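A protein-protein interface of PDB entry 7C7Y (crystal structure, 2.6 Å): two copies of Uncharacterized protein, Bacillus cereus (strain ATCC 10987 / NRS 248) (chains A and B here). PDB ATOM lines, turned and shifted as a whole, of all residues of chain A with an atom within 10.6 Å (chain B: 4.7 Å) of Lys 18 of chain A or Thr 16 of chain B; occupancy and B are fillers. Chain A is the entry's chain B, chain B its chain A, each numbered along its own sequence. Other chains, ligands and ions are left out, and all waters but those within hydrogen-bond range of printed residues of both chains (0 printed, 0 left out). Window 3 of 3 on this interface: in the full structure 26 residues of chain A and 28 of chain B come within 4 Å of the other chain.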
ATOM      1  N   ASP A  10      -1.030 -19.838   6.851  1.00  0.00           N
ATOM      2  CA  ASP A  10      -1.787 -19.078   5.829  1.00  0.00           C
ATOM      3  C   ASP A  10      -3.202 -18.846   6.347  1.00  0.00           C
ATOM      4  O   ASP A  10      -3.696 -17.719   6.226  1.00  0.00           O
ATOM      5  CB  ASP A  10      -1.739 -19.783   4.479  1.00  0.00           C
ATOM      6  CG  ASP A  10      -0.328 -19.846   3.931  1.00  0.00           C
ATOM      7  OD1 ASP A  10       0.492 -18.976   4.314  1.00  0.00           O
ATOM      8  OD2 ASP A  10      -0.053 -20.778   3.159  1.00  0.00           O
ATOM      9  N   PHE A  11      -3.802 -19.856   6.960  1.00  0.00           N
ATOM     10  CA  PHE A  11      -5.181 -19.742   7.489  1.00  0.00           C
ATOM     11  C   PHE A  11      -5.197 -18.743   8.648  1.00  0.00           C
ATOM     12  O   PHE A  11      -6.047 -17.848   8.662  1.00  0.00           O
ATOM     13  CB  PHE A  11      -5.738 -21.096   7.937  1.00  0.00           C
ATOM     14  CG  PHE A  11      -6.990 -20.990   8.774  1.00  0.00           C
ATOM     15  CD1 PHE A  11      -8.211 -20.741   8.182  1.00  0.00           C
ATOM     16  CD2 PHE A  11      -6.942 -21.110  10.155  1.00  0.00           C
ATOM     17  CE1 PHE A  11      -9.356 -20.624   8.955  1.00  0.00           C
ATOM     18  CE2 PHE A  11      -8.085 -20.976  10.925  1.00  0.00           C
ATOM     19  CZ  PHE A  11      -9.291 -20.734  10.321  1.00  0.00           C
ATOM     20  N   ILE A  12      -4.328 -18.935   9.630  1.00  0.00           N
ATOM     21  CA  ILE A  12      -4.250 -18.031  10.814  1.00  0.00           C
ATOM     22  C   ILE A  12      -4.020 -16.599  10.319  1.00  0.00           C
ATOM     23  O   ILE A  12      -4.686 -15.695  10.820  1.00  0.00           O
ATOM     24  CB  ILE A  12      -3.143 -18.457  11.793  1.00  0.00           C
ATOM     25  CG1 ILE A  12      -3.451 -19.776  12.502  1.00  0.00           C
ATOM     26  CG2 ILE A  12      -2.903 -17.348  12.786  1.00  0.00           C
ATOM     27  CD1 ILE A  12      -4.620 -19.696  13.452  1.00  0.00           C
ATOM     28  N   GLU A  13      -3.077 -16.406   9.399  1.00  0.00           N
ATOM     29  CA  GLU A  13      -2.719 -15.074   8.863  1.00  0.00           C
ATOM     30  C   GLU A  13      -3.982 -14.449   8.309  1.00  0.00           C
ATOM     31  O   GLU A  13      -4.375 -13.355   8.780  1.00  0.00           O
ATOM     32  CB  GLU A  13      -1.717 -15.160   7.711  1.00  0.00           C
ATOM     33  CG  GLU A  13      -0.287 -14.954   8.155  1.00  0.00           C
ATOM     34  CD  GLU A  13       0.754 -15.646   7.295  1.00  0.00           C
ATOM     35  OE1 GLU A  13       0.598 -15.652   6.039  1.00  0.00           O
ATOM     36  OE2 GLU A  13       1.709 -16.196   7.896  1.00  0.00           O
ATOM     37  N   ALA A  14      -4.555 -15.155   7.341  1.00  0.00           N
ATOM     38  CA  ALA A  14      -5.747 -14.750   6.576  1.00  0.00           C
ATOM     39  C   ALA A  14      -6.808 -14.301   7.568  1.00  0.00           C
ATOM     40  O   ALA A  14      -7.315 -13.185   7.375  1.00  0.00           O
ATOM     41  CB  ALA A  14      -6.240 -15.882   5.711  1.00  0.00           C
ATOM     42  N   LEU A  15      -7.060 -15.119   8.606  1.00  0.00           N
ATOM     43  CA  LEU A  15      -8.130 -14.892   9.617  1.00  0.00           C
ATOM     44  C   LEU A  15      -7.765 -13.667  10.455  1.00  0.00           C
ATOM     45  O   LEU A  15      -8.646 -12.840  10.728  1.00  0.00           O
ATOM     46  CB  LEU A  15      -8.269 -16.138  10.497  1.00  0.00           C
ATOM     47  CG  LEU A  15      -9.251 -16.025  11.656  1.00  0.00           C
ATOM     48  CD1 LEU A  15     -10.589 -15.527  11.176  1.00  0.00           C
ATOM     49  CD2 LEU A  15      -9.417 -17.365  12.348  1.00  0.00           C
ATOM     50  N   THR A  16      -6.498 -13.554  10.834  1.00  0.00           N
ATOM     51  CA  THR A  16      -6.016 -12.430  11.661  1.00  0.00           C
ATOM     52  C   THR A  16      -6.216 -11.118  10.895  1.00  0.00           C
ATOM     53  O   THR A  16      -6.813 -10.161  11.456  1.00  0.00           O
ATOM     54  CB  THR A  16      -4.586 -12.692  12.112  1.00  0.00           C
ATOM     55  OG1 THR A  16      -4.673 -13.819  12.996  1.00  0.00           O
ATOM     56  CG2 THR A  16      -3.997 -11.487  12.806  1.00  0.00           C
ATOM     57  N   GLU A  17      -5.801 -11.066   9.640  1.00  0.00           N
ATOM     58  CA  GLU A  17      -5.927  -9.817   8.862  1.00  0.00           C
ATOM     59  C   GLU A  17      -7.400  -9.419   8.832  1.00  0.00           C
ATOM     60  O   GLU A  17      -7.731  -8.313   9.275  1.00  0.00           O
ATOM     61  CB  GLU A  17      -5.343 -10.005   7.467  1.00  0.00           C
ATOM     62  CG  GLU A  17      -5.040  -8.691   6.783  1.00  0.00           C
ATOM     63  CD  GLU A  17      -4.618  -8.807   5.327  1.00  0.00           C
ATOM     64  OE1 GLU A  17      -4.038  -9.860   4.951  1.00  0.00           O
ATOM     65  OE2 GLU A  17      -4.868  -7.838   4.571  1.00  0.00           O
ATOM     66  N   LYS A  18      -8.280 -10.316   8.395  1.00  0.00           N
ATOM     67  CA  LYS A  18      -9.686  -9.946   8.087  1.00  0.00           C
ATOM     68  C   LYS A  18     -10.366  -9.436   9.364  1.00  0.00           C
ATOM     69  O   LYS A  18     -10.965  -8.316   9.306  1.00  0.00           O
ATOM     70  CB  LYS A  18     -10.434 -11.125   7.462  1.00  0.00           C
ATOM     71  CG  LYS A  18     -11.700 -10.765   6.689  1.00  0.00           C
ATOM     72  CD  LYS A  18     -11.623 -11.126   5.219  1.00  0.00           C
ATOM     73  CE  LYS A  18     -12.867 -10.751   4.439  1.00  0.00           C
ATOM     74  NZ  LYS A  18     -12.977  -9.282   4.272  1.00  0.00           N
ATOM     75  N   ILE A  19     -10.246 -10.182  10.483  1.00  0.00           N
ATOM     76  CA  ILE A  19     -10.853  -9.803  11.801  1.00  0.00           C
ATOM     77  C   ILE A  19     -10.473  -8.347  12.111  1.00  0.00           C
ATOM     78  O   ILE A  19     -11.375  -7.558  12.414  1.00  0.00           O
ATOM     79  CB  ILE A  19     -10.420 -10.753  12.930  1.00  0.00           C
ATOM     80  CG1 ILE A  19     -10.977 -12.166  12.749  1.00  0.00           C
ATOM     81  CG2 ILE A  19     -10.816 -10.183  14.291  1.00  0.00           C
ATOM     82  CD1 ILE A  19     -10.525 -13.160  13.833  1.00  0.00           C
ATOM     83  N   THR A  20      -9.190  -7.988  11.964  1.00  0.00           N
ATOM     84  CA  THR A  20      -8.638  -6.686  12.415  1.00  0.00           C
ATOM     85  C   THR A  20      -9.157  -5.560  11.523  1.00  0.00           C
ATOM     86  O   THR A  20      -9.692  -4.591  12.084  1.00  0.00           O
ATOM     87  CB  THR A  20      -7.114  -6.737  12.473  1.00  0.00           C
ATOM     88  OG1 THR A  20      -6.812  -7.760  13.415  1.00  0.00           O
ATOM     89  CG2 THR A  20      -6.469  -5.446  12.918  1.00  0.00           C
ATOM     90  N   GLU A  21      -9.003  -5.680  10.204  1.00  0.00           N
ATOM     91  CA  GLU A  21      -9.648  -4.780   9.211  1.00  0.00           C
ATOM     92  C   GLU A  21     -11.133  -4.606   9.566  1.00  0.00           C
ATOM     93  O   GLU A  21     -11.549  -3.455   9.850  1.00  0.00           O
ATOM     94  CB  GLU A  21      -9.531  -5.364   7.805  1.00  0.00           C
ATOM     95  CG  GLU A  21      -8.255  -4.999   7.066  1.00  0.00           C
ATOM     96  CD  GLU A  21      -8.520  -4.489   5.652  1.00  0.00           C
ATOM     97  OE1 GLU A  21      -9.278  -5.170   4.904  1.00  0.00           O
ATOM     98  OE2 GLU A  21      -7.992  -3.394   5.300  1.00  0.00           O
ATOM     99  N   GLU A  22     -11.893  -5.703   9.575  1.00  0.00           N
ATOM    100  CA  GLU A  22     -13.368  -5.678   9.675  1.00  0.00           C
ATOM    101  C   GLU A  22     -13.811  -5.119  11.027  1.00  0.00           C
ATOM    102  O   GLU A  22     -14.752  -4.269  11.032  1.00  0.00           O
ATOM    103  CB  GLU A  22     -13.964  -7.066   9.448  1.00  0.00           C
ATOM    104  CG  GLU A  22     -14.102  -7.441   7.977  1.00  0.00           C
ATOM    105  CD  GLU A  22     -14.683  -6.358   7.084  1.00  0.00           C
ATOM    106  OE1 GLU A  22     -15.701  -5.785   7.485  1.00  0.00           O
ATOM    107  OE2 GLU A  22     -14.099  -6.067   5.999  1.00  0.00           O
ATOM    108  N   VAL A  23     -13.228  -5.583  12.136  1.00  0.00           N
ATOM    109  CA  VAL A  23     -13.704  -5.139  13.471  1.00  0.00           C
ATOM    110  C   VAL A  23     -13.438  -3.635  13.533  1.00  0.00           C
ATOM    111  O   VAL A  23     -14.349  -2.865  13.888  1.00  0.00           O
ATOM    112  CB  VAL A  23     -13.026  -5.889  14.626  1.00  0.00           C
ATOM    113  CG1 VAL A  23     -13.300  -5.205  15.959  1.00  0.00           C
ATOM    114  CG2 VAL A  23     -13.455  -7.351  14.700  1.00  0.00           C
ATOM    115  N   THR A  24     -12.221  -3.235  13.186  1.00  0.00           N
ATOM    116  CA  THR A  24     -11.829  -1.801  13.158  1.00  0.00           C
ATOM    117  C   THR A  24     -12.791  -0.983  12.286  1.00  0.00           C
ATOM    118  O   THR A  24     -13.421  -0.044  12.808  1.00  0.00           O
ATOM    119  CB  THR A  24     -10.400  -1.614  12.655  1.00  0.00           C
ATOM    120  OG1 THR A  24      -9.573  -2.383  13.525  1.00  0.00           O
ATOM    121  CG2 THR A  24     -10.003  -0.159  12.671  1.00  0.00           C
ATOM    122  N   ALA A  25     -12.878  -1.303  10.999  1.00  0.00           N
ATOM    123  CA  ALA A  25     -13.826  -0.643  10.068  1.00  0.00           C
ATOM    124  C   ALA A  25     -15.221  -0.574  10.697  1.00  0.00           C
ATOM    125  O   ALA A  25     -15.752   0.520  10.808  1.00  0.00           O
ATOM    126  CB  ALA A  25     -13.858  -1.363   8.745  1.00  0.00           C
ATOM    127  N   LYS A  26     -15.788  -1.698  11.117  1.00  0.00           N
ATOM    128  CA  LYS A  26     -17.205  -1.739  11.561  1.00  0.00           C
ATOM    129  C   LYS A  26     -17.364  -0.864  12.813  1.00  0.00           C
ATOM    130  O   LYS A  26     -18.342  -0.132  12.890  1.00  0.00           O
ATOM    131  CB  LYS A  26     -17.618  -3.194  11.784  1.00  0.00           C
ATOM    132  CG  LYS A  26     -19.006  -3.395  12.369  1.00  0.00           C
ATOM    133  CD  LYS A  26     -20.147  -3.263  11.377  1.00  0.00           C
ATOM    134  CE  LYS A  26     -21.478  -3.700  11.968  1.00  0.00           C
ATOM    135  NZ  LYS A  26     -22.615  -3.351  11.086  1.00  0.00           N
ATOM    136  N   VAL A  27     -16.431  -0.933  13.766  1.00  0.00           N
ATOM    137  CA  VAL A  27     -16.536  -0.207  15.067  1.00  0.00           C
ATOM    138  C   VAL A  27     -16.393   1.299  14.809  1.00  0.00           C
ATOM    139  O   VAL A  27     -17.355   2.050  15.134  1.00  0.00           O
ATOM    140  CB  VAL A  27     -15.521  -0.730  16.098  1.00  0.00           C
ATOM    141  CG1 VAL A  27     -15.305   0.250  17.237  1.00  0.00           C
ATOM    142  CG2 VAL A  27     -15.961  -2.063  16.677  1.00  0.00           C
ATOM    143  N   ILE B  12     -13.773 -18.327   6.926  1.00  0.00           N
ATOM    144  CA  ILE B  12     -13.010 -17.129   7.400  1.00  0.00           C
ATOM    145  C   ILE B  12     -13.940 -15.905   7.419  1.00  0.00           C
ATOM    146  O   ILE B  12     -13.966 -15.154   8.432  1.00  0.00           O
ATOM    147  CB  ILE B  12     -11.812 -16.859   6.467  1.00  0.00           C
ATOM    148  CG1 ILE B  12     -10.766 -17.979   6.472  1.00  0.00           C
ATOM    149  CG2 ILE B  12     -11.201 -15.505   6.781  1.00  0.00           C
ATOM    150  CD1 ILE B  12      -9.732 -17.859   7.547  1.00  0.00           C
ATOM    151  N   GLU B  13     -14.633 -15.702   6.300  1.00  0.00           N
ATOM    152  CA  GLU B  13     -15.568 -14.585   6.044  1.00  0.00           C
ATOM    153  C   GLU B  13     -16.703 -14.659   7.079  1.00  0.00           C
ATOM    154  O   GLU B  13     -17.195 -13.584   7.525  1.00  0.00           O
ATOM    155  CB  GLU B  13     -16.016 -14.728   4.580  1.00  0.00           C
ATOM    156  CG  GLU B  13     -16.609 -13.487   3.933  1.00  0.00           C
ATOM    157  CD  GLU B  13     -17.153 -13.738   2.529  1.00  0.00           C
ATOM    158  OE1 GLU B  13     -16.492 -14.488   1.768  1.00  0.00           O
ATOM    159  OE2 GLU B  13     -18.242 -13.198   2.193  1.00  0.00           O
ATOM    160  N   ALA B  14     -17.103 -15.876   7.471  1.00  0.00           N
ATOM    161  CA  ALA B  14     -18.269 -16.092   8.355  1.00  0.00           C
ATOM    162  C   ALA B  14     -17.833 -15.808   9.785  1.00  0.00           C
ATOM    163  O   ALA B  14     -18.559 -15.060  10.471  1.00  0.00           O
ATOM    164  CB  ALA B  14     -18.860 -17.483   8.225  1.00  0.00           C
ATOM    165  N   LEU B  15     -16.717 -16.414  10.213  1.00  0.00           N
ATOM    166  CA  LEU B  15     -16.117 -16.111  11.533  1.00  0.00           C
ATOM    167  C   LEU B  15     -15.929 -14.593  11.624  1.00  0.00           C
ATOM    168  O   LEU B  15     -16.278 -14.006  12.639  1.00  0.00           O
ATOM    169  CB  LEU B  15     -14.776 -16.810  11.660  1.00  0.00           C
ATOM    170  CG  LEU B  15     -14.770 -18.122  12.426  1.00  0.00           C
ATOM    171  CD1 LEU B  15     -13.333 -18.615  12.567  1.00  0.00           C
ATOM    172  CD2 LEU B  15     -15.427 -17.958  13.793  1.00  0.00           C
ATOM    173  N   THR B  16     -15.452 -13.949  10.560  1.00  0.00           N
ATOM    174  CA  THR B  16     -15.111 -12.518  10.659  1.00  0.00           C
ATOM    175  C   THR B  16     -16.397 -11.720  10.851  1.00  0.00           C
ATOM    176  O   THR B  16     -16.392 -10.888  11.746  1.00  0.00           O
ATOM    177  CB  THR B  16     -14.228 -12.033   9.513  1.00  0.00           C
ATOM    178  OG1 THR B  16     -12.945 -12.670   9.591  1.00  0.00           O
ATOM    179  CG2 THR B  16     -14.042 -10.537   9.584  1.00  0.00           C
ATOM    180  N   GLU B  17     -17.470 -11.993  10.107  1.00  0.00           N
ATOM    181  CA  GLU B  17     -18.744 -11.237  10.266  1.00  0.00           C
ATOM    182  C   GLU B  17     -19.338 -11.510  11.655  1.00  0.00           C
ATOM    183  O   GLU B  17     -19.938 -10.591  12.248  1.00  0.00           O
ATOM    184  CB  GLU B  17     -19.767 -11.573   9.188  1.00  0.00           C
ATOM    185  CG  GLU B  17     -21.043 -10.775   9.360  1.00  0.00           C
ATOM    186  CD  GLU B  17     -21.729 -10.383   8.069  1.00  0.00           C
ATOM    187  OE1 GLU B  17     -21.044 -10.379   7.030  1.00  0.00           O
ATOM    188  OE2 GLU B  17     -22.940 -10.068   8.111  1.00  0.00           O
ATOM    189  N   LYS B  18     -19.162 -12.710  12.183  1.00  0.00           N
ATOM    190  CA  LYS B  18     -19.708 -13.014  13.521  1.00  0.00           C
ATOM    191  C   LYS B  18     -18.958 -12.210  14.572  1.00  0.00           C
ATOM    192  O   LYS B  18     -19.602 -11.434  15.275  1.00  0.00           O
ATOM    193  CB  LYS B  18     -19.607 -14.480  13.918  1.00  0.00           C
ATOM    194  CG  LYS B  18     -20.334 -14.765  15.222  1.00  0.00           C
ATOM    195  CD  LYS B  18     -19.632 -15.736  16.130  1.00  0.00           C
ATOM    196  CE  LYS B  18     -20.467 -16.071  17.351  1.00  0.00           C
ATOM    197  NZ  LYS B  18     -19.865 -17.172  18.132  1.00  0.00           N
ATOM    198  N   ILE B  19     -17.653 -12.415  14.700  1.00  0.00           N
ATOM    199  CA  ILE B  19     -16.827 -11.630  15.666  1.00  0.00           C
ATOM    200  C   ILE B  19     -17.214 -10.153  15.491  1.00  0.00           C
ATOM    201  O   ILE B  19     -17.670  -9.544  16.461  1.00  0.00           O
ATOM    202  CB  ILE B  19     -15.313 -11.890  15.488  1.00  0.00           C
ATOM    203  CG1 ILE B  19     -14.973 -13.376  15.647  1.00  0.00           C
ATOM    204  CG2 ILE B  19     -14.496 -11.042  16.459  1.00  0.00           C
ATOM    205  CD1 ILE B  19     -13.524 -13.719  15.351  1.00  0.00           C
ATOM    206  N   THR B  20     -17.133  -9.625  14.270  1.00  0.00           N
ATOM    207  CA  THR B  20     -17.288  -8.177  13.992  1.00  0.00           C
ATOM    208  C   THR B  20     -18.591  -7.653  14.595  1.00  0.00           C
ATOM    209  O   THR B  20     -18.574  -6.522  15.107  1.00  0.00           O
ATOM    210  CB  THR B  20     -17.200  -7.890  12.493  1.00  0.00           C
ATOM    211  OG1 THR B  20     -15.886  -8.284  12.084  1.00  0.00           O
ATOM    212  CG2 THR B  20     -17.405  -6.430  12.166  1.00  0.00           C
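Among the printed residues, pairs that only touch across the chains: Phe 11 of chain A with Ile 12 of chain B (3.1 Å), Leu 15 of chain A with Ile 12 of chain B (3.7 Å), Lys 18 of chain A with Thr 16 of chain B (3.6 Å), Ile 19 of chain A with Thr 16 of chain B (3.8 Å), Ile 19 of chain A with Ile 19 of chain B (3.4 Å), Glu 22 of chain A with Thr 16 of chain B (3.5 Å), Glu 22 of chain A with Thr 20 of chain B (3.5 Å), Val 23 of chain A with Thr 20 of chain B (3.7 Å) and Lys 26 of chain A with Thr 20 of chain B (3.3 Å).
Lys 18 of chain A touches just one residue of chain B: Thr 16 (3.6 Å).
Ile 12 of chain B touches just these residues of chain A: Phe 11 and Leu 15.
No residue of chain A comes within 4 Å of Glu 13 of chain B.
No residue of chain A comes within 4 Å of Ala 14 of chain B.
Leu 15 of chain B touches none of the printed residues of chain A.
Of the printed residues of chain A, Ile 19 of chain B touches Ile 19 (3.4 Å).
Thr 20 of chain B touches three residues of chain A.
Printed residues of chain B within 4 Å of Ile 19 of chain A: Thr 16 (3.8 Å) and Ile 19 (3.4 Å).
Printed residues of chain B within 4 Å of Lys 26 of chain A: Thr 20 (3.3 Å).
Thr 16 of chain A touches none of the printed residues of chain B.
The nearest residue of chain A that does not touch Thr 16 of chain B is Leu 15 of chain A (4.03 Å).
The nearest printed residue of chain B that does not touch Leu 15 of chain A is Thr 16 of chain B (4.03 Å).
NZ of Lys 18 of chain A is in salt-bridge range of OE2 of Glu 22 of chain A (3.8 Å).
The backbone carbonyl oxygen (O) of Ile 12 of chain B sits at hydrogen-bond distance from the side-chain hydroxyl (OG1) of Thr 16 of chain B, at 2.9 Å.
The side-chain hydroxyl (OG1) of Thr 20 of chain B is in hydrogen-bond range of the backbone carbonyl oxygen (O) of Thr 16 of chain B (2.7 Å).
Hydrophobic or aromatic side chains of chain A that line the printed part of chain B: Phe 11, Leu 15, Ile 19 and Val 23.
Printed residues of chain B that touch a printed residue of chain A: Ile 12, Thr 16, Ile 19 and Thr 20.
Hydrophobic or aromatic side chains of chain B within 4 Å of the printed part of chain A: Ile 12 and Ile 19.
Among the printed residues, no Asp or Glu carboxylate lies within 4 Å of a Lys or Arg side-chain nitrogen of the other chain.
Leu 15 of chain A touches Ile 12 of chain B, but with the chains exchanged Ile 12 of chain A does not touch Leu 15 of chain B (8.8 Å).
Lys 18 of chain A touches Thr 16 of chain B, but with the chains exchanged Thr 16 of chain A does not touch Lys 18 of chain B (12.6 Å).
Ile 19 of chain A touches Thr 16 of chain B, but with the chains exchanged Thr 16 of chain A does not touch Ile 19 of chain B (8.4 Å).
Ile 19 of chain A touches its own counterpart, Ile 19 of chain B.
9 positions are printed for both chains.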
